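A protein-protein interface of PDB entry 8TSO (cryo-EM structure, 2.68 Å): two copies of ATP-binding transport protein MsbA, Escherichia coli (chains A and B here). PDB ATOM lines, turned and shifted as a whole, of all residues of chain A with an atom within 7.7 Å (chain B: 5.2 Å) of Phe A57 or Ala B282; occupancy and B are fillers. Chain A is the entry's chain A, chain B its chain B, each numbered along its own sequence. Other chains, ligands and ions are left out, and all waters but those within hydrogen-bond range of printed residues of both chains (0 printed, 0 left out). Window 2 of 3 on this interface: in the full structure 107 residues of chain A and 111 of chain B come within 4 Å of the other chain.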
ATOM      1  N   PRO A  51       7.873 -22.632  28.945  1.00  0.00           N
ATOM      2  CA  PRO A  51       7.651 -21.782  30.125  1.00  0.00           C
ATOM      3  C   PRO A  51       6.825 -20.541  29.828  1.00  0.00           C
ATOM      4  O   PRO A  51       5.940 -20.184  30.610  1.00  0.00           O
ATOM      5  CB  PRO A  51       9.074 -21.407  30.569  1.00  0.00           C
ATOM      6  CG  PRO A  51       9.966 -21.781  29.429  1.00  0.00           C
ATOM      7  CD  PRO A  51       9.304 -22.937  28.771  1.00  0.00           C
ATOM      8  N   LEU A  52       7.086 -19.892  28.692  1.00  0.00           N
ATOM      9  CA  LEU A  52       6.371 -18.663  28.357  1.00  0.00           C
ATOM     10  C   LEU A  52       4.886 -18.926  28.149  1.00  0.00           C
ATOM     11  O   LEU A  52       4.035 -18.153  28.603  1.00  0.00           O
ATOM     12  CB  LEU A  52       6.980 -18.020  27.111  1.00  0.00           C
ATOM     13  CG  LEU A  52       8.298 -17.267  27.292  1.00  0.00           C
ATOM     14  CD1 LEU A  52       8.806 -16.758  25.953  1.00  0.00           C
ATOM     15  CD2 LEU A  52       8.123 -16.120  28.271  1.00  0.00           C
ATOM     16  N   LEU A  53       4.552 -20.013  27.452  1.00  0.00           N
ATOM     17  CA  LEU A  53       3.149 -20.295  27.167  1.00  0.00           C
ATOM     18  C   LEU A  53       2.420 -20.816  28.399  1.00  0.00           C
ATOM     19  O   LEU A  53       1.258 -20.463  28.632  1.00  0.00           O
ATOM     20  CB  LEU A  53       3.039 -21.287  26.011  1.00  0.00           C
ATOM     21  CG  LEU A  53       3.550 -20.778  24.661  1.00  0.00           C
ATOM     22  CD1 LEU A  53       3.530 -21.887  23.623  1.00  0.00           C
ATOM     23  CD2 LEU A  53       2.733 -19.587  24.189  1.00  0.00           C
ATOM     24  N   ASP A  54       3.079 -21.652  29.203  1.00  0.00           N
ATOM     25  CA  ASP A  54       2.415 -22.251  30.355  1.00  0.00           C
ATOM     26  C   ASP A  54       2.389 -21.307  31.551  1.00  0.00           C
ATOM     27  O   ASP A  54       1.313 -20.897  31.998  1.00  0.00           O
ATOM     28  CB  ASP A  54       3.099 -23.565  30.737  1.00  0.00           C
ATOM     29  CG  ASP A  54       3.083 -24.578  29.613  1.00  0.00           C
ATOM     30  OD1 ASP A  54       2.585 -24.245  28.517  1.00  0.00           O
ATOM     31  OD2 ASP A  54       3.566 -25.711  29.823  1.00  0.00           O
ATOM     32  N   ASP A  55       3.565 -20.957  32.076  1.00  0.00           N
ATOM     33  CA  ASP A  55       3.619 -20.096  33.253  1.00  0.00           C
ATOM     34  C   ASP A  55       3.133 -18.689  32.927  1.00  0.00           C
ATOM     35  O   ASP A  55       2.389 -18.080  33.705  1.00  0.00           O
ATOM     36  CB  ASP A  55       5.042 -20.062  33.810  1.00  0.00           C
ATOM     37  CG  ASP A  55       5.567 -21.441  34.148  1.00  0.00           C
ATOM     38  OD1 ASP A  55       4.829 -22.427  33.939  1.00  0.00           O
ATOM     39  OD2 ASP A  55       6.718 -21.540  34.623  1.00  0.00           O
ATOM     40  N   GLY A  56       3.540 -18.160  31.785  1.00  0.00           N
ATOM     41  CA  GLY A  56       3.174 -16.822  31.369  1.00  0.00           C
ATOM     42  C   GLY A  56       4.292 -15.824  31.622  1.00  0.00           C
ATOM     43  O   GLY A  56       5.274 -16.094  32.314  1.00  0.00           O
ATOM     44  N   PHE A  57       4.119 -14.647  31.030  1.00  0.00           N
ATOM     45  CA  PHE A  57       5.069 -13.563  31.213  1.00  0.00           C
ATOM     46  C   PHE A  57       5.007 -13.039  32.643  1.00  0.00           C
ATOM     47  O   PHE A  57       3.940 -12.971  33.259  1.00  0.00           O
ATOM     48  CB  PHE A  57       4.797 -12.426  30.227  1.00  0.00           C
ATOM     49  CG  PHE A  57       5.154 -12.752  28.802  1.00  0.00           C
ATOM     50  CD1 PHE A  57       4.474 -13.736  28.105  1.00  0.00           C
ATOM     51  CD2 PHE A  57       6.169 -12.068  28.159  1.00  0.00           C
ATOM     52  CE1 PHE A  57       4.801 -14.031  26.798  1.00  0.00           C
ATOM     53  CE2 PHE A  57       6.501 -12.360  26.852  1.00  0.00           C
ATOM     54  CZ  PHE A  57       5.817 -13.342  26.171  1.00  0.00           C
ATOM     55  N   GLY A  58       6.175 -12.663  33.169  1.00  0.00           N
ATOM     56  CA  GLY A  58       6.323 -12.198  34.532  1.00  0.00           C
ATOM     57  C   GLY A  58       7.184 -13.103  35.391  1.00  0.00           C
ATOM     58  O   GLY A  58       7.892 -12.611  36.278  1.00  0.00           O
ATOM     59  N   LYS A  59       7.139 -14.411  35.147  1.00  0.00           N
ATOM     60  CA  LYS A  59       7.974 -15.370  35.853  1.00  0.00           C
ATOM     61  C   LYS A  59       9.321 -15.588  35.178  1.00  0.00           C
ATOM     62  O   LYS A  59      10.153 -16.328  35.709  1.00  0.00           O
ATOM     63  CB  LYS A  59       7.242 -16.710  35.986  1.00  0.00           C
ATOM     64  CG  LYS A  59       5.833 -16.593  36.538  1.00  0.00           C
ATOM     65  CD  LYS A  59       5.223 -17.960  36.791  1.00  0.00           C
ATOM     66  CE  LYS A  59       3.792 -17.839  37.288  1.00  0.00           C
ATOM     67  NZ  LYS A  59       2.926 -17.108  36.321  1.00  0.00           N
ATOM     68  N   THR A  60       9.553 -14.965  34.029  1.00  0.00           N
ATOM     69  CA  THR A  60      10.797 -15.101  33.290  1.00  0.00           C
ATOM     70  C   THR A  60      11.731 -13.940  33.613  1.00  0.00           C
ATOM     71  O   THR A  60      11.296 -12.822  33.901  1.00  0.00           O
ATOM     72  CB  THR A  60      10.526 -15.160  31.782  1.00  0.00           C
ATOM     73  OG1 THR A  60       9.374 -15.976  31.536  1.00  0.00           O
ATOM     74  CG2 THR A  60      11.718 -15.754  31.044  1.00  0.00           C
ATOM     75  N   LEU A  65      14.674 -11.864  28.493  1.00  0.00           N
ATOM     76  CA  LEU A  65      13.661 -11.318  27.597  1.00  0.00           C
ATOM     77  C   LEU A  65      14.254 -10.324  26.607  1.00  0.00           C
ATOM     78  O   LEU A  65      13.711 -10.142  25.512  1.00  0.00           O
ATOM     79  CB  LEU A  65      12.548 -10.659  28.412  1.00  0.00           C
ATOM     80  CG  LEU A  65      11.134 -10.730  27.840  1.00  0.00           C
ATOM     81  CD1 LEU A  65      10.802 -12.147  27.410  1.00  0.00           C
ATOM     82  CD2 LEU A  65      10.130 -10.233  28.863  1.00  0.00           C
ATOM     83  N   MET A  68      15.634 -12.508  23.904  1.00  0.00           N
ATOM     84  CA  MET A  68      14.652 -13.389  23.275  1.00  0.00           C
ATOM     85  C   MET A  68      14.342 -13.055  21.817  1.00  0.00           C
ATOM     86  O   MET A  68      14.284 -13.994  21.005  1.00  0.00           O
ATOM     87  CB  MET A  68      13.358 -13.392  24.102  1.00  0.00           C
ATOM     88  CG  MET A  68      13.405 -14.263  25.344  1.00  0.00           C
ATOM     89  SD  MET A  68      13.212 -16.018  24.986  1.00  0.00           S
ATOM     90  CE  MET A  68      14.912 -16.571  25.097  1.00  0.00           C
ATOM     91  N   VAL B 267       6.700  -8.324  20.135  1.00  0.00           N
ATOM     92  CA  VAL B 267       5.975  -8.512  21.390  1.00  0.00           C
ATOM     93  C   VAL B 267       6.942  -8.814  22.525  1.00  0.00           C
ATOM     94  O   VAL B 267       6.812  -8.276  23.632  1.00  0.00           O
ATOM     95  CB  VAL B 267       4.915  -9.618  21.234  1.00  0.00           C
ATOM     96  CG1 VAL B 267       4.465 -10.124  22.594  1.00  0.00           C
ATOM     97  CG2 VAL B 267       3.737  -9.094  20.449  1.00  0.00           C
ATOM     98  N   LEU B 268       7.931  -9.675  22.273  1.00  0.00           N
ATOM     99  CA  LEU B 268       8.922  -9.982  23.298  1.00  0.00           C
ATOM    100  C   LEU B 268       9.762  -8.761  23.653  1.00  0.00           C
ATOM    101  O   LEU B 268      10.098  -8.564  24.825  1.00  0.00           O
ATOM    102  CB  LEU B 268       9.820 -11.129  22.839  1.00  0.00           C
ATOM    103  CG  LEU B 268       9.180 -12.518  22.846  1.00  0.00           C
ATOM    104  CD1 LEU B 268       9.968 -13.471  21.968  1.00  0.00           C
ATOM    105  CD2 LEU B 268       9.069 -13.058  24.260  1.00  0.00           C
ATOM    106  N   ALA B 271       7.634  -6.596  25.844  1.00  0.00           N
ATOM    107  CA  ALA B 271       7.449  -7.199  27.159  1.00  0.00           C
ATOM    108  C   ALA B 271       8.660  -7.039  28.065  1.00  0.00           C
ATOM    109  O   ALA B 271       8.560  -7.353  29.255  1.00  0.00           O
ATOM    110  CB  ALA B 271       7.110  -8.682  27.012  1.00  0.00           C
ATOM    111  N   MET B 277       4.692  -3.494  30.637  1.00  0.00           N
ATOM    112  CA  MET B 277       4.206  -4.771  31.149  1.00  0.00           C
ATOM    113  C   MET B 277       3.226  -4.608  32.299  1.00  0.00           C
ATOM    114  O   MET B 277       2.220  -5.319  32.346  1.00  0.00           O
ATOM    115  CB  MET B 277       5.384  -5.654  31.593  1.00  0.00           C
ATOM    116  CG  MET B 277       4.962  -6.904  32.353  1.00  0.00           C
ATOM    117  SD  MET B 277       5.010  -8.406  31.357  1.00  0.00           S
ATOM    118  CE  MET B 277       6.753  -8.805  31.430  1.00  0.00           C
ATOM    119  N   LEU B 280      -0.246  -3.371  30.935  1.00  0.00           N
ATOM    120  CA  LEU B 280      -1.043  -4.380  30.249  1.00  0.00           C
ATOM    121  C   LEU B 280      -1.329  -5.602  31.113  1.00  0.00           C
ATOM    122  O   LEU B 280      -1.695  -6.650  30.573  1.00  0.00           O
ATOM    123  CB  LEU B 280      -0.349  -4.811  28.952  1.00  0.00           C
ATOM    124  CG  LEU B 280      -0.069  -3.751  27.881  1.00  0.00           C
ATOM    125  CD1 LEU B 280      -0.173  -4.367  26.501  1.00  0.00           C
ATOM    126  CD2 LEU B 280      -1.018  -2.567  27.986  1.00  0.00           C
ATOM    127  N   THR B 281      -1.155  -5.495  32.428  1.00  0.00           N
ATOM    128  CA  THR B 281      -1.495  -6.488  33.449  1.00  0.00           C
ATOM    129  C   THR B 281      -0.657  -7.758  33.347  1.00  0.00           C
ATOM    130  O   THR B 281      -0.860  -8.669  34.162  1.00  0.00           O
ATOM    131  CB  THR B 281      -2.981  -6.885  33.429  1.00  0.00           C
ATOM    132  OG1 THR B 281      -3.245  -7.713  32.288  1.00  0.00           O
ATOM    133  CG2 THR B 281      -3.871  -5.650  33.377  1.00  0.00           C
ATOM    134  N   ALA B 282       0.260  -7.862  32.383  1.00  0.00           N
ATOM    135  CA  ALA B 282       1.139  -9.024  32.216  1.00  0.00           C
ATOM    136  C   ALA B 282       0.357 -10.318  32.005  1.00  0.00           C
ATOM    137  O   ALA B 282       0.921 -11.413  32.094  1.00  0.00           O
ATOM    138  CB  ALA B 282       2.098  -9.173  33.402  1.00  0.00           C
ATOM    139  N   GLY B 283      -0.938 -10.215  31.722  1.00  0.00           N
ATOM    140  CA  GLY B 283      -1.757 -11.383  31.470  1.00  0.00           C
ATOM    141  C   GLY B 283      -2.321 -11.372  30.068  1.00  0.00           C
ATOM    142  O   GLY B 283      -2.589 -12.427  29.486  1.00  0.00           O
ATOM    143  N   THR B 284      -2.513 -10.172  29.518  1.00  0.00           N
ATOM    144  CA  THR B 284      -2.917 -10.044  28.126  1.00  0.00           C
ATOM    145  C   THR B 284      -1.753 -10.289  27.176  1.00  0.00           C
ATOM    146  O   THR B 284      -1.964 -10.748  26.049  1.00  0.00           O
ATOM    147  CB  THR B 284      -3.514  -8.658  27.874  1.00  0.00           C
ATOM    148  OG1 THR B 284      -2.465  -7.684  27.842  1.00  0.00           O
ATOM    149  CG2 THR B 284      -4.497  -8.297  28.975  1.00  0.00           C
ATOM    150  N   ILE B 285      -0.527  -9.994  27.617  1.00  0.00           N
ATOM    151  CA  ILE B 285       0.646 -10.189  26.769  1.00  0.00           C
ATOM    152  C   ILE B 285       0.836 -11.666  26.455  1.00  0.00           C
ATOM    153  O   ILE B 285       1.159 -12.038  25.319  1.00  0.00           O
ATOM    154  CB  ILE B 285       1.891  -9.585  27.444  1.00  0.00           C
ATOM    155  CG1 ILE B 285       1.671  -8.095  27.722  1.00  0.00           C
ATOM    156  CG2 ILE B 285       3.122  -9.800  26.581  1.00  0.00           C
ATOM    157  CD1 ILE B 285       2.944  -7.282  27.800  1.00  0.00           C
ATOM    158  N   THR B 286       0.645 -12.529  27.455  1.00  0.00           N
ATOM    159  CA  THR B 286       0.754 -13.966  27.227  1.00  0.00           C
ATOM    160  C   THR B 286      -0.291 -14.445  26.229  1.00  0.00           C
ATOM    161  O   THR B 286       0.006 -15.262  25.349  1.00  0.00           O
ATOM    162  CB  THR B 286       0.606 -14.716  28.551  1.00  0.00           C
ATOM    163  OG1 THR B 286       1.493 -14.149  29.524  1.00  0.00           O
ATOM    164  CG2 THR B 286       0.932 -16.190  28.372  1.00  0.00           C
ATOM    165  N   PHE B 289       0.742 -13.304  22.735  1.00  0.00           N
ATOM    166  CA  PHE B 289       1.855 -14.111  22.246  1.00  0.00           C
ATOM    167  C   PHE B 289       1.377 -15.489  21.798  1.00  0.00           C
ATOM    168  O   PHE B 289       1.761 -15.978  20.726  1.00  0.00           O
ATOM    169  CB  PHE B 289       2.919 -14.226  23.339  1.00  0.00           C
ATOM    170  CG  PHE B 289       4.255 -14.696  22.846  1.00  0.00           C
ATOM    171  CD1 PHE B 289       5.062 -13.856  22.100  1.00  0.00           C
ATOM    172  CD2 PHE B 289       4.716 -15.963  23.151  1.00  0.00           C
ATOM    173  CE1 PHE B 289       6.293 -14.279  21.649  1.00  0.00           C
ATOM    174  CE2 PHE B 289       5.950 -16.389  22.707  1.00  0.00           C
ATOM    175  CZ  PHE B 289       6.739 -15.547  21.954  1.00  0.00           C
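Of the 12 printed residues of chain A, 4 touch a printed residue of chain B. Hydrophobic or aromatic side chains of chain A that line the printed part of chain B: Phe A57 and Leu A65. Hydrophobic or aromatic side chains of chain B within 4 Å of the printed part of chain A: Leu B268, Ala B271 and Phe B289. Among the printed residues, 9 pairs touch across the chains. Among the printed residues, no Asp or Glu carboxylate lies within 4 Å of a Lys or Arg side-chain nitrogen of the other chain.
Among the printed residues, merely in contact across the chains: Leu A52 with Thr B286 (3.7 Å), Gly A56 with Thr B286 (3.7 Å), Phe A57 with Leu B268 (3.7 Å), Phe A57 with Ala B271 (3.7 Å), Phe A57 with Ala B282 (3.6 Å), Phe A57 with Phe B289 (3.9 Å), Leu A65 with Leu B268 (3.7 Å) and Leu A65 with Ala B271 (3.3 Å).
N of Phe A57 sits at hydrogen-bond distance from OG1 of Thr B286 (3.1 Å).
No position is printed for both chains.
Of chain B, only Leu B268, Ala B271, Ala B282, Thr B286 and Phe B289 come within 4 Å of Phe A57. Ala B282 touches one residue of chain A. Printed residues of chain A within 4 Å of Thr B286: Leu A52 (3.7 Å), Gly A56 (3.7 Å) and Phe A57 (3.1 Å). Of the printed residues of chain B, Leu A65 touches Leu B268 and Ala B271. Of the printed residues of chain B, Gly A56 touches Thr B286. Of the printed residues of chain B, Leu A52 touches Thr B286 (3.7 Å). Of the printed residues of chain A, Ala B271 touches Phe A57 (3.7 Å) and Leu A65 (3.3 Å). Lys A59 touches none of the printed residues of chain B.
The backbone carbonyl oxygen (O) of Pro A51 is in hydrogen-bond range of the backbone NH (N) of Gly A56 (3.4 Å). The backbone carbonyl oxygen (O) of Met B277 is in hydrogen-bond range of the backbone NH (N) of Ala B282.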
